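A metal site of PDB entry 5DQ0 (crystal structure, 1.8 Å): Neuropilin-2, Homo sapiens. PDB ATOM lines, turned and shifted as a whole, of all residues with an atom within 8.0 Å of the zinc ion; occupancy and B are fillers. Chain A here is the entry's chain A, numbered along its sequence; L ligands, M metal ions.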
ATOM      1  N   LEU A  92     -14.986   9.535 -17.730  1.00  0.00           N
ATOM      2  CA  LEU A  92     -13.704  10.003 -18.137  1.00  0.00           C
ATOM      3  C   LEU A  92     -13.171  10.897 -17.026  1.00  0.00           C
ATOM      4  O   LEU A  92     -13.911  11.739 -16.536  1.00  0.00           O
ATOM      5  CB  LEU A  92     -13.854  10.817 -19.406  1.00  0.00           C
ATOM      6  CG  LEU A  92     -12.757  11.694 -19.941  1.00  0.00           C
ATOM      7  CD1 LEU A  92     -11.546  10.903 -20.408  1.00  0.00           C
ATOM      8  CD2 LEU A  92     -13.277  12.609 -21.043  1.00  0.00           C
ATOM      9  N   TYR A 104     -15.018  14.262 -15.822  1.00  0.00           N
ATOM     10  CA  TYR A 104     -15.620  15.060 -16.869  1.00  0.00           C
ATOM     11  C   TYR A 104     -17.156  15.116 -16.682  1.00  0.00           C
ATOM     12  O   TYR A 104     -17.795  14.066 -16.507  1.00  0.00           O
ATOM     13  CB  TYR A 104     -15.278  14.520 -18.255  1.00  0.00           C
ATOM     14  CG  TYR A 104     -15.905  15.307 -19.400  1.00  0.00           C
ATOM     15  CD1 TYR A 104     -15.632  16.648 -19.584  1.00  0.00           C
ATOM     16  CD2 TYR A 104     -16.773  14.710 -20.295  1.00  0.00           C
ATOM     17  CE1 TYR A 104     -16.226  17.375 -20.618  1.00  0.00           C
ATOM     18  CE2 TYR A 104     -17.398  15.422 -21.337  1.00  0.00           C
ATOM     19  CZ  TYR A 104     -17.116  16.759 -21.502  1.00  0.00           C
ATOM     20  OH  TYR A 104     -17.660  17.518 -22.526  1.00  0.00           O
ATOM     21  N   ARG A 105     -17.673  16.339 -16.666  1.00  0.00           N
ATOM     22  CA  ARG A 105     -19.109  16.568 -16.379  1.00  0.00           C
ATOM     23  C   ARG A 105     -19.735  17.527 -17.362  1.00  0.00           C
ATOM     24  O   ARG A 105     -19.085  18.311 -18.013  1.00  0.00           O
ATOM     25  CB  ARG A 105     -19.391  17.051 -14.956  1.00  0.00           C
ATOM     26  CG  ARG A 105     -18.430  17.983 -14.364  1.00  0.00           C
ATOM     27  CD  ARG A 105     -18.770  18.250 -12.891  1.00  0.00           C
ATOM     28  NE  ARG A 105     -18.123  19.520 -12.584  1.00  0.00           N
ATOM     29  CZ  ARG A 105     -16.884  19.663 -12.104  1.00  0.00           C
ATOM     30  NH1 ARG A 105     -16.101  18.611 -11.782  1.00  0.00           N
ATOM     31  NH2 ARG A 105     -16.424  20.896 -11.901  1.00  0.00           N
ATOM     32  N   HIS A 106     -21.059  17.424 -17.449  1.00  0.00           N
ATOM     33  CA  HIS A 106     -21.913  18.438 -18.040  1.00  0.00           C
ATOM     34  C   HIS A 106     -22.701  19.050 -16.866  1.00  0.00           C
ATOM     35  O   HIS A 106     -23.474  18.323 -16.211  1.00  0.00           O
ATOM     36  CB  HIS A 106     -22.875  17.737 -19.010  1.00  0.00           C
ATOM     37  CG  HIS A 106     -22.234  17.252 -20.255  1.00  0.00           C
ATOM     38  ND1 HIS A 106     -22.940  16.543 -21.196  1.00  0.00           N
ATOM     39  CD2 HIS A 106     -20.986  17.420 -20.773  1.00  0.00           C
ATOM     40  CE1 HIS A 106     -22.158  16.292 -22.241  1.00  0.00           C
ATOM     41  NE2 HIS A 106     -20.971  16.802 -21.994  1.00  0.00           N
ATOM     42  N   LYS A 111     -20.439  12.976 -16.996  1.00  0.00           N
ATOM     43  CA  LYS A 111     -20.803  12.449 -18.303  1.00  0.00           C
ATOM     44  C   LYS A 111     -20.585  10.953 -18.353  1.00  0.00           C
ATOM     45  O   LYS A 111     -19.486  10.461 -18.137  1.00  0.00           O
ATOM     46  CB  LYS A 111     -20.040  13.214 -19.373  1.00  0.00           C
ATOM     47  CG  LYS A 111     -20.241  12.690 -20.785  1.00  0.00           C
ATOM     48  CD  LYS A 111     -21.679  12.724 -21.279  1.00  0.00           C
ATOM     49  CE  LYS A 111     -21.746  12.124 -22.715  1.00  0.00           C
ATOM     50  NZ  LYS A 111     -23.152  12.172 -23.201  1.00  0.00           N
ATOM     51  N   PHE A 113     -20.456   7.977 -20.803  1.00  0.00           N
ATOM     52  CA  PHE A 113     -20.395   7.630 -22.222  1.00  0.00           C
ATOM     53  C   PHE A 113     -20.952   6.214 -22.414  1.00  0.00           C
ATOM     54  O   PHE A 113     -20.576   5.304 -21.720  1.00  0.00           O
ATOM     55  CB  PHE A 113     -18.950   7.729 -22.741  1.00  0.00           C
ATOM     56  CG  PHE A 113     -18.408   9.131 -22.713  1.00  0.00           C
ATOM     57  CD1 PHE A 113     -18.552   9.966 -23.806  1.00  0.00           C
ATOM     58  CD2 PHE A 113     -17.673   9.583 -21.633  1.00  0.00           C
ATOM     59  CE1 PHE A 113     -18.013  11.231 -23.829  1.00  0.00           C
ATOM     60  CE2 PHE A 113     -17.171  10.890 -21.622  1.00  0.00           C
ATOM     61  CZ  PHE A 113     -17.337  11.706 -22.704  1.00  0.00           C
ATOM     62  N   LYS A 126     -17.799  11.249 -29.805  1.00  0.00           N
ATOM     63  CA  LYS A 126     -17.227  12.565 -29.980  1.00  0.00           C
ATOM     64  C   LYS A 126     -17.615  13.448 -28.782  1.00  0.00           C
ATOM     65  O   LYS A 126     -18.756  13.414 -28.352  1.00  0.00           O
ATOM     66  CB  LYS A 126     -17.690  13.197 -31.290  1.00  0.00           C
ATOM     67  CG  LYS A 126     -17.303  12.355 -32.508  1.00  0.00           C
ATOM     68  CD  LYS A 126     -17.753  13.015 -33.818  1.00  0.00           C
ATOM     69  CE  LYS A 126     -17.200  12.254 -35.033  1.00  0.00           C
ATOM     70  NZ  LYS A 126     -17.930  12.606 -36.277  1.00  0.00           N
ATOM     71  N   LEU A 127     -16.694  14.236 -28.250  1.00  0.00           N
ATOM     72  CA  LEU A 127     -17.029  15.191 -27.194  1.00  0.00           C
ATOM     73  C   LEU A 127     -17.756  16.392 -27.773  1.00  0.00           C
ATOM     74  O   LEU A 127     -17.469  16.830 -28.883  1.00  0.00           O
ATOM     75  CB  LEU A 127     -15.776  15.630 -26.456  1.00  0.00           C
ATOM     76  CG  LEU A 127     -15.299  14.666 -25.339  1.00  0.00           C
ATOM     77  CD1 LEU A 127     -14.806  13.343 -25.872  1.00  0.00           C
ATOM     78  CD2 LEU A 127     -14.153  15.338 -24.645  1.00  0.00           C
ATOM     79  N   HIS A 128     -18.647  17.004 -26.997  1.00  0.00           N
ATOM     80  CA  HIS A 128     -19.453  18.112 -27.519  1.00  0.00           C
ATOM     81  C   HIS A 128     -18.628  19.338 -27.805  1.00  0.00           C
ATOM     82  O   HIS A 128     -19.037  20.191 -28.604  1.00  0.00           O
ATOM     83  CB  HIS A 128     -20.614  18.421 -26.563  1.00  0.00           C
ATOM     84  CG  HIS A 128     -20.238  19.315 -25.445  1.00  0.00           C
ATOM     85  ND1 HIS A 128     -19.663  18.867 -24.280  1.00  0.00           N
ATOM     86  CD2 HIS A 128     -20.329  20.664 -25.335  1.00  0.00           C
ATOM     87  CE1 HIS A 128     -19.401  19.904 -23.506  1.00  0.00           C
ATOM     88  NE2 HIS A 128     -19.807  21.008 -24.119  1.00  0.00           N
ATOM     89  N   ALA A 129     -17.502  19.476 -27.126  1.00  0.00           N
ATOM     90  CA  ALA A 129     -16.531  20.505 -27.378  1.00  0.00           C
ATOM     91  C   ALA A 129     -15.180  19.990 -26.956  1.00  0.00           C
ATOM     92  O   ALA A 129     -15.081  19.082 -26.154  1.00  0.00           O
ATOM     93  CB  ALA A 129     -16.886  21.791 -26.622  1.00  0.00           C
ATOM     94  N   PRO A 130     -14.103  20.528 -27.521  1.00  0.00           N
ATOM     95  CA  PRO A 130     -12.821  19.943 -27.167  1.00  0.00           C
ATOM     96  C   PRO A 130     -12.450  20.178 -25.663  1.00  0.00           C
ATOM     97  O   PRO A 130     -12.842  21.170 -25.049  1.00  0.00           O
ATOM     98  CB  PRO A 130     -11.871  20.660 -28.101  1.00  0.00           C
ATOM     99  CG  PRO A 130     -12.711  21.231 -29.213  1.00  0.00           C
ATOM    100  CD  PRO A 130     -13.982  21.582 -28.545  1.00  0.00           C
ATOM    101  N   LEU A 131     -11.803  19.184 -25.086  1.00  0.00           N
ATOM    102  CA  LEU A 131     -11.510  19.180 -23.661  1.00  0.00           C
ATOM    103  C   LEU A 131      -9.999  19.210 -23.464  1.00  0.00           C
ATOM    104  O   LEU A 131      -9.308  18.362 -24.023  1.00  0.00           O
ATOM    105  CB  LEU A 131     -12.098  17.923 -23.075  1.00  0.00           C
ATOM    106  CG  LEU A 131     -11.774  17.497 -21.633  1.00  0.00           C
ATOM    107  CD1 LEU A 131     -12.231  18.627 -20.709  1.00  0.00           C
ATOM    108  CD2 LEU A 131     -12.421  16.159 -21.267  1.00  0.00           C
HETATM  109 CL1  LIG L   1     -19.484  15.241 -24.480  1.00  0.00          CL
HETATM  110 ZN    ZN M   1     -19.334  17.036 -23.326  1.00  0.00          ZN
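O of Tyr 104 sits at hydrogen-bond distance from N of Lys 111 (2.9 Å). O of Leu 92 lies within hydrogen-bond range of N of Tyr 104 (2.8 Å).
The zinc ion is bound by the side-chain hydroxyl (OH) of Tyr 104 (1.9 Å). A ring nitrogen (ND1) of His 128 is bound to the zinc ion (2.1 Å). The zinc ion is bound by NE2 of His 106, 2.1 Å away. A chlorine (CL1) of the ligand binds the zinc ion (2.1 Å).
Within 4 Å of the zinc ion: Tyr 104, His 106 and His 128. Along chain A the residues within 4 Å of the zinc ion span positions 104 to 128.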
